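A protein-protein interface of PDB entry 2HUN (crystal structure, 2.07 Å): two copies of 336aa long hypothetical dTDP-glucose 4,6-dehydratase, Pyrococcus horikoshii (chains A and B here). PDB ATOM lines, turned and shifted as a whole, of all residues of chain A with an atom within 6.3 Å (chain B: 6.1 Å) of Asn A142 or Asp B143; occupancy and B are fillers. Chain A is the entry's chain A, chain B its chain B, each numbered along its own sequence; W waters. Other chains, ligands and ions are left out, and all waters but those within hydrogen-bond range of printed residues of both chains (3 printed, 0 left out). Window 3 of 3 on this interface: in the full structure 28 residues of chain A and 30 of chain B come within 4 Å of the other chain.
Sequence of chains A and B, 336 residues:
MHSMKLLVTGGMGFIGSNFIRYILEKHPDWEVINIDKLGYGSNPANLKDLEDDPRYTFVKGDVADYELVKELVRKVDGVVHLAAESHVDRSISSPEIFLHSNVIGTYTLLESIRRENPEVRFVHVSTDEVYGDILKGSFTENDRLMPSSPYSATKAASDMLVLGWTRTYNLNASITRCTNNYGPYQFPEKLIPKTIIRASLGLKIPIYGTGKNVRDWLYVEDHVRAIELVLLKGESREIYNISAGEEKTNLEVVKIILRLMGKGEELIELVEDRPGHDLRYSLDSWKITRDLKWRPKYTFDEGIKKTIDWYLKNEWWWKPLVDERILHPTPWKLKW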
ATOM      1  N   TYR A 131      -4.332  -6.763  26.907  1.00  0.00           N
ATOM      2  CA  TYR A 131      -4.803  -5.546  26.248  1.00  0.00           C
ATOM      3  C   TYR A 131      -6.302  -5.493  25.954  1.00  0.00           C
ATOM      4  O   TYR A 131      -6.832  -4.437  25.614  1.00  0.00           O
ATOM      5  CB  TYR A 131      -4.130  -5.389  24.886  1.00  0.00           C
ATOM      6  CG  TYR A 131      -2.621  -5.277  24.914  1.00  0.00           C
ATOM      7  CD1 TYR A 131      -1.996  -4.077  25.261  1.00  0.00           C
ATOM      8  CD2 TYR A 131      -1.821  -6.360  24.557  1.00  0.00           C
ATOM      9  CE1 TYR A 131      -0.607  -3.957  25.241  1.00  0.00           C
ATOM     10  CE2 TYR A 131      -0.430  -6.256  24.534  1.00  0.00           C
ATOM     11  CZ  TYR A 131       0.169  -5.049  24.876  1.00  0.00           C
ATOM     12  OH  TYR A 131       1.537  -4.932  24.846  1.00  0.00           O
ATOM     13  N   PHE A 139      -2.348  -3.316  19.235  1.00  0.00           N
ATOM     14  CA  PHE A 139      -1.806  -2.732  20.456  1.00  0.00           C
ATOM     15  C   PHE A 139      -0.282  -2.775  20.515  1.00  0.00           C
ATOM     16  O   PHE A 139       0.343  -3.778  20.147  1.00  0.00           O
ATOM     17  CB  PHE A 139      -2.356  -3.475  21.686  1.00  0.00           C
ATOM     18  CG  PHE A 139      -3.818  -3.230  21.953  1.00  0.00           C
ATOM     19  CD1 PHE A 139      -4.263  -1.980  22.370  1.00  0.00           C
ATOM     20  CD2 PHE A 139      -4.749  -4.259  21.818  1.00  0.00           C
ATOM     21  CE1 PHE A 139      -5.610  -1.757  22.649  1.00  0.00           C
ATOM     22  CE2 PHE A 139      -6.104  -4.044  22.095  1.00  0.00           C
ATOM     23  CZ  PHE A 139      -6.533  -2.793  22.511  1.00  0.00           C
ATOM     24  N   THR A 140       0.322  -1.683  20.978  1.00  0.00           N
ATOM     25  CA  THR A 140       1.768  -1.653  21.119  1.00  0.00           C
ATOM     26  C   THR A 140       2.014  -1.797  22.615  1.00  0.00           C
ATOM     27  O   THR A 140       1.081  -1.697  23.416  1.00  0.00           O
ATOM     28  CB  THR A 140       2.397  -0.330  20.662  1.00  0.00           C
ATOM     29  OG1 THR A 140       2.200   0.656  21.676  1.00  0.00           O
ATOM     30  CG2 THR A 140       1.775   0.150  19.354  1.00  0.00           C
ATOM     31  N   GLU A 141       3.264  -2.034  22.983  1.00  0.00           N
ATOM     32  CA  GLU A 141       3.627  -2.193  24.385  1.00  0.00           C
ATOM     33  C   GLU A 141       3.418  -0.891  25.162  1.00  0.00           C
ATOM     34  O   GLU A 141       3.510  -0.878  26.388  1.00  0.00           O
ATOM     35  CB  GLU A 141       5.092  -2.652  24.506  1.00  0.00           C
ATOM     36  CG  GLU A 141       5.406  -3.969  23.794  1.00  0.00           C
ATOM     37  CD  GLU A 141       5.678  -3.810  22.301  1.00  0.00           C
ATOM     38  OE1 GLU A 141       5.489  -2.709  21.752  1.00  0.00           O
ATOM     39  OE2 GLU A 141       6.080  -4.803  21.667  1.00  0.00           O
ATOM     40  N   ASN A 142       3.129   0.205  24.459  1.00  0.00           N
ATOM     41  CA  ASN A 142       2.894   1.475  25.159  1.00  0.00           C
ATOM     42  C   ASN A 142       1.415   1.774  25.413  1.00  0.00           C
ATOM     43  O   ASN A 142       1.081   2.821  25.962  1.00  0.00           O
ATOM     44  CB  ASN A 142       3.527   2.646  24.390  1.00  0.00           C
ATOM     45  CG  ASN A 142       5.044   2.612  24.432  1.00  0.00           C
ATOM     46  OD1 ASN A 142       5.634   2.227  25.441  1.00  0.00           O
ATOM     47  ND2 ASN A 142       5.683   3.027  23.343  1.00  0.00           N
ATOM     48  N   ASP A 143       0.531   0.857  25.027  1.00  0.00           N
ATOM     49  CA  ASP A 143      -0.904   1.057  25.235  1.00  0.00           C
ATOM     50  C   ASP A 143      -1.357   0.505  26.579  1.00  0.00           C
ATOM     51  O   ASP A 143      -0.753  -0.414  27.111  1.00  0.00           O
ATOM     52  CB  ASP A 143      -1.704   0.383  24.119  1.00  0.00           C
ATOM     53  CG  ASP A 143      -1.465   1.025  22.769  1.00  0.00           C
ATOM     54  OD1 ASP A 143      -1.348   2.259  22.726  1.00  0.00           O
ATOM     55  OD2 ASP A 143      -1.416   0.300  21.754  1.00  0.00           O
ATOM     56  N   ARG A 144      -2.422   1.082  27.125  1.00  0.00           N
ATOM     57  CA  ARG A 144      -2.971   0.652  28.401  1.00  0.00           C
ATOM     58  C   ARG A 144      -3.466  -0.775  28.270  1.00  0.00           C
ATOM     59  O   ARG A 144      -3.664  -1.277  27.167  1.00  0.00           O
ATOM     60  CB  ARG A 144      -4.160   1.538  28.805  1.00  0.00           C
ATOM     61  CG  ARG A 144      -5.505   1.154  28.125  1.00  0.00           C
ATOM     62  CD  ARG A 144      -5.473   1.339  26.599  1.00  0.00           C
ATOM     63  NE  ARG A 144      -6.730   0.934  25.965  1.00  0.00           N
ATOM     64  CZ  ARG A 144      -7.126  -0.327  25.794  1.00  0.00           C
ATOM     65  NH1 ARG A 144      -6.363  -1.336  26.202  1.00  0.00           N
ATOM     66  NH2 ARG A 144      -8.300  -0.585  25.226  1.00  0.00           N
ATOM     67  N   LEU A 145      -3.680  -1.423  29.406  1.00  0.00           N
ATOM     68  CA  LEU A 145      -4.200  -2.773  29.406  1.00  0.00           C
ATOM     69  C   LEU A 145      -5.692  -2.663  29.710  1.00  0.00           C
ATOM     70  O   LEU A 145      -6.147  -1.659  30.264  1.00  0.00           O
ATOM     71  CB  LEU A 145      -3.504  -3.623  30.479  1.00  0.00           C
ATOM     72  CG  LEU A 145      -1.974  -3.723  30.378  1.00  0.00           C
ATOM     73  CD1 LEU A 145      -1.454  -4.717  31.403  1.00  0.00           C
ATOM     74  CD2 LEU A 145      -1.571  -4.140  28.990  1.00  0.00           C
ATOM     75  N   LYS A 287       8.392  -3.674  17.803  1.00  0.00           N
ATOM     76  CA  LYS A 287       9.483  -3.445  18.750  1.00  0.00           C
ATOM     77  C   LYS A 287      10.530  -4.555  18.721  1.00  0.00           C
ATOM     78  O   LYS A 287      11.720  -4.296  18.545  1.00  0.00           O
ATOM     79  CB  LYS A 287       8.919  -3.297  20.164  1.00  0.00           C
ATOM     80  CG  LYS A 287       9.951  -2.989  21.250  1.00  0.00           C
ATOM     81  CD  LYS A 287       9.244  -2.712  22.571  1.00  0.00           C
ATOM     82  CE  LYS A 287      10.209  -2.392  23.691  1.00  0.00           C
ATOM     83  NZ  LYS A 287       9.472  -2.122  24.961  1.00  0.00           N
ATOM     84  N   TYR B 131       1.843   5.363  36.349  1.00  0.00           N
ATOM     85  CA  TYR B 131       2.345   5.608  34.988  1.00  0.00           C
ATOM     86  C   TYR B 131       3.860   5.754  34.967  1.00  0.00           C
ATOM     87  O   TYR B 131       4.501   5.647  33.916  1.00  0.00           O
ATOM     88  CB  TYR B 131       1.742   6.880  34.401  1.00  0.00           C
ATOM     89  CG  TYR B 131       0.244   6.872  34.248  1.00  0.00           C
ATOM     90  CD1 TYR B 131      -0.369   6.290  33.133  1.00  0.00           C
ATOM     91  CD2 TYR B 131      -0.563   7.505  35.189  1.00  0.00           C
ATOM     92  CE1 TYR B 131      -1.755   6.351  32.961  1.00  0.00           C
ATOM     93  CE2 TYR B 131      -1.939   7.571  35.028  1.00  0.00           C
ATOM     94  CZ  TYR B 131      -2.529   6.994  33.915  1.00  0.00           C
ATOM     95  OH  TYR B 131      -3.892   7.065  33.779  1.00  0.00           O
ATOM     96  N   SER B 138       2.195  14.614  29.339  1.00  0.00           N
ATOM     97  CA  SER B 138       1.397  14.014  30.413  1.00  0.00           C
ATOM     98  C   SER B 138       0.760  12.710  29.930  1.00  0.00           C
ATOM     99  O   SER B 138       0.535  12.543  28.736  1.00  0.00           O
ATOM    100  CB  SER B 138       0.273  14.973  30.829  1.00  0.00           C
ATOM    101  OG  SER B 138       0.767  16.233  31.260  1.00  0.00           O
ATOM    102  N   PHE B 139       0.447  11.812  30.865  1.00  0.00           N
ATOM    103  CA  PHE B 139      -0.175  10.526  30.541  1.00  0.00           C
ATOM    104  C   PHE B 139      -1.700  10.598  30.533  1.00  0.00           C
ATOM    105  O   PHE B 139      -2.301  11.261  31.378  1.00  0.00           O
ATOM    106  CB  PHE B 139       0.231   9.458  31.566  1.00  0.00           C
ATOM    107  CG  PHE B 139       1.682   9.065  31.507  1.00  0.00           C
ATOM    108  CD1 PHE B 139       2.163   8.284  30.460  1.00  0.00           C
ATOM    109  CD2 PHE B 139       2.559   9.438  32.522  1.00  0.00           C
ATOM    110  CE1 PHE B 139       3.499   7.875  30.425  1.00  0.00           C
ATOM    111  CE2 PHE B 139       3.902   9.031  32.498  1.00  0.00           C
ATOM    112  CZ  PHE B 139       4.368   8.249  31.448  1.00  0.00           C
ATOM    113  N   THR B 140      -2.315   9.903  29.579  1.00  0.00           N
ATOM    114  CA  THR B 140      -3.767   9.834  29.483  1.00  0.00           C
ATOM    115  C   THR B 140      -4.120   8.442  30.014  1.00  0.00           C
ATOM    116  O   THR B 140      -3.234   7.600  30.216  1.00  0.00           O
ATOM    117  CB  THR B 140      -4.275   9.909  28.023  1.00  0.00           C
ATOM    118  OG1 THR B 140      -4.092   8.635  27.401  1.00  0.00           O
ATOM    119  CG2 THR B 140      -3.501  10.961  27.225  1.00  0.00           C
ATOM    120  N   GLU B 141      -5.407   8.202  30.228  1.00  0.00           N
ATOM    121  CA  GLU B 141      -5.859   6.916  30.736  1.00  0.00           C
ATOM    122  C   GLU B 141      -5.596   5.794  29.722  1.00  0.00           C
ATOM    123  O   GLU B 141      -5.687   4.617  30.060  1.00  0.00           O
ATOM    124  CB  GLU B 141      -7.359   6.986  31.080  1.00  0.00           C
ATOM    125  CG  GLU B 141      -7.727   8.001  32.181  1.00  0.00           C
ATOM    126  CD  GLU B 141      -7.819   9.441  31.692  1.00  0.00           C
ATOM    127  OE1 GLU B 141      -7.605   9.694  30.490  1.00  0.00           O
ATOM    128  OE2 GLU B 141      -8.111  10.334  32.517  1.00  0.00           O
ATOM    129  N   ASN B 142      -5.259   6.152  28.484  1.00  0.00           N
ATOM    130  CA  ASN B 142      -4.992   5.133  27.471  1.00  0.00           C
ATOM    131  C   ASN B 142      -3.518   4.724  27.373  1.00  0.00           C
ATOM    132  O   ASN B 142      -3.152   3.899  26.538  1.00  0.00           O
ATOM    133  CB  ASN B 142      -5.491   5.591  26.098  1.00  0.00           C
ATOM    134  CG  ASN B 142      -6.993   5.768  26.061  1.00  0.00           C
ATOM    135  OD1 ASN B 142      -7.709   5.199  26.883  1.00  0.00           O
ATOM    136  ND2 ASN B 142      -7.481   6.546  25.101  1.00  0.00           N
ATOM    137  N   ASP B 143      -2.678   5.288  28.232  1.00  0.00           N
ATOM    138  CA  ASP B 143      -1.259   4.949  28.209  1.00  0.00           C
ATOM    139  C   ASP B 143      -0.903   3.813  29.159  1.00  0.00           C
ATOM    140  O   ASP B 143      -1.560   3.611  30.180  1.00  0.00           O
ATOM    141  CB  ASP B 143      -0.411   6.173  28.550  1.00  0.00           C
ATOM    142  CG  ASP B 143      -0.484   7.245  27.481  1.00  0.00           C
ATOM    143  OD1 ASP B 143      -0.528   6.892  26.287  1.00  0.00           O
ATOM    144  OD2 ASP B 143      -0.490   8.435  27.834  1.00  0.00           O
ATOM    145  N   ARG B 144       0.147   3.077  28.798  1.00  0.00           N
ATOM    146  CA  ARG B 144       0.642   1.964  29.592  1.00  0.00           C
ATOM    147  C   ARG B 144       1.098   2.470  30.952  1.00  0.00           C
ATOM    148  O   ARG B 144       1.358   3.665  31.132  1.00  0.00           O
ATOM    149  CB  ARG B 144       1.846   1.311  28.901  1.00  0.00           C
ATOM    150  CG  ARG B 144       3.196   2.008  29.194  1.00  0.00           C
ATOM    151  CD  ARG B 144       3.275   3.450  28.645  1.00  0.00           C
ATOM    152  NE  ARG B 144       4.585   4.059  28.906  1.00  0.00           N
ATOM    153  CZ  ARG B 144       4.993   4.498  30.094  1.00  0.00           C
ATOM    154  NH1 ARG B 144       4.191   4.417  31.146  1.00  0.00           N
ATOM    155  NH2 ARG B 144       6.224   4.972  30.247  1.00  0.00           N
ATOM    156  N   LEU B 145       1.204   1.551  31.903  1.00  0.00           N
ATOM    157  CA  LEU B 145       1.670   1.883  33.234  1.00  0.00           C
ATOM    158  C   LEU B 145       3.141   1.475  33.281  1.00  0.00           C
ATOM    159  O   LEU B 145       3.589   0.678  32.456  1.00  0.00           O
ATOM    160  CB  LEU B 145       0.872   1.112  34.294  1.00  0.00           C
ATOM    161  CG  LEU B 145      -0.652   1.285  34.238  1.00  0.00           C
ATOM    162  CD1 LEU B 145      -1.282   0.661  35.491  1.00  0.00           C
ATOM    163  CD2 LEU B 145      -1.017   2.760  34.148  1.00  0.00           C
ATOM    164  N   ARG B 177      -7.241   8.221  39.394  1.00  0.00           N
ATOM    165  CA  ARG B 177      -5.807   8.342  39.606  1.00  0.00           C
ATOM    166  C   ARG B 177      -5.501   9.832  39.747  1.00  0.00           C
ATOM    167  O   ARG B 177      -5.582  10.591  38.777  1.00  0.00           O
ATOM    168  CB  ARG B 177      -5.033   7.752  38.422  1.00  0.00           C
ATOM    169  CG  ARG B 177      -5.143   6.232  38.307  1.00  0.00           C
ATOM    170  CD  ARG B 177      -4.622   5.719  36.974  1.00  0.00           C
ATOM    171  NE  ARG B 177      -4.636   4.256  36.926  1.00  0.00           N
ATOM    172  CZ  ARG B 177      -4.468   3.539  35.824  1.00  0.00           C
ATOM    173  NH1 ARG B 177      -4.273   4.141  34.654  1.00  0.00           N
ATOM    174  NH2 ARG B 177      -4.493   2.213  35.892  1.00  0.00           N
HETATM  175  O   HOH W   1       6.532   1.733  27.773  1.00  0.00           O
HETATM  176  O   HOH W   2      -8.865   2.899  27.707  1.00  0.00           O
HETATM  177  O   HOH W   3      -3.187   3.735  23.748  1.00  0.00           O
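Glu A141 touches Arg B144, and with the chains exchanged Arg A144 touches Glu B141. Asn A142 touches Asp B143, and with the chains exchanged Asp A143 touches Asn B142. Asn A142 touches Arg B144, and with the chains exchanged Arg A144 touches Asn B142. Arg A144 touches its own counterpart, Arg B144. Positions printed for both chains: 131, 139, 140, 141, 142, 143, 144 and 145.
The side-chain hydroxyl of Thr B140 lies within hydrogen-bond range of the backbone NH of Asn B142. The backbone NH (N) of Thr A140 lies within hydrogen-bond range of the side-chain carboxylate (OD2) of Asp A143. The backbone carbonyl oxygen (O) of Tyr A131 lies within hydrogen-bond range of the guanidinium group (NH1) of Arg A144. The backbone NH (N) of Thr B140 lies within hydrogen-bond range of the side-chain carboxylate (OD2) of Asp B143 (2.9 Å). N of Asn A142 lies close to OG1 of Thr A140 (3.0 Å). The guanidinium group (NH1) of Arg B144 lies within hydrogen-bond range of the backbone carbonyl oxygen (O) of Tyr B131 (3.0 Å).
The backbone carbonyl oxygen of Asn A142 is in hydrogen-bond range of the backbone NH of Arg B144, 3.0 Å away. The backbone NH (N) of Arg A144 sits at hydrogen-bond distance from the backbone carbonyl oxygen (O) of Asn B142, 3.0 Å away.
Printed residues of chain A that touch a printed residue of chain B: Glu A141, Asn A142, Asp A143 and Arg A144. Of the 10 printed residues of chain B, 4 touch a printed residue of chain A. Among the printed residues, 9 pairs touch across the chains. Among the printed residues, no Asp or Glu carboxylate lies within 4 Å of a Lys or Arg side-chain nitrogen of the other chain.
Glu A141 touches Arg B144. O of Asn A142 touches CA of Asp B143 (3.9 Å). Asp A143 touches Asn B142 (C to O, 3.8 Å). O of Asp A143 touches CB of Arg B144, at 3.6 Å. CB of Arg A144 touches O of Glu B141, 3.7 Å away. Asp B143 touches Arg A144. Arg B144 touches Arg A144.
Water W1 bridges OD1 of Asn A142 (2.5 Å) and NE of Arg B144 (3.2 Å). Water W3 bridges the side-chain carboxylate (OD1) of Asp A143 (2.6 Å) and the backbone carbonyl oxygen (O) of Asn B142 (2.8 Å). Water W2 bridges the side-chain amide oxygen of Asn B142 and the guanidinium group of Arg A144.
Asn A142 touches just these residues of chain B: Asp B143 and Arg B144. Of chain A, only Asn A142 (3.9 Å) and Arg A144 (3.6 Å) come within 4 Å of Asp B143. Of the printed residues of chain B, Arg A144 touches Glu B141, Asn B142, Asp B143 and Arg B144. Of the printed residues of chain A, Arg B144 touches Glu A141 (3.7 Å), Asn A142 (3.0 Å), Asp A143 (3.6 Å) and Arg A144 (3.7 Å). Of the printed residues of chain B, Asp A143 touches Asn B142 and Arg B144. Of the printed residues of chain B, Glu A141 touches Arg B144 (3.7 Å). Printed residues of chain A within 4 Å of Asn B142: Asp A143 (3.8 Å) and Arg A144 (3.0 Å). The nearest residue of chain A that does not touch Asp B143 is Asp A143 (4.2 Å).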
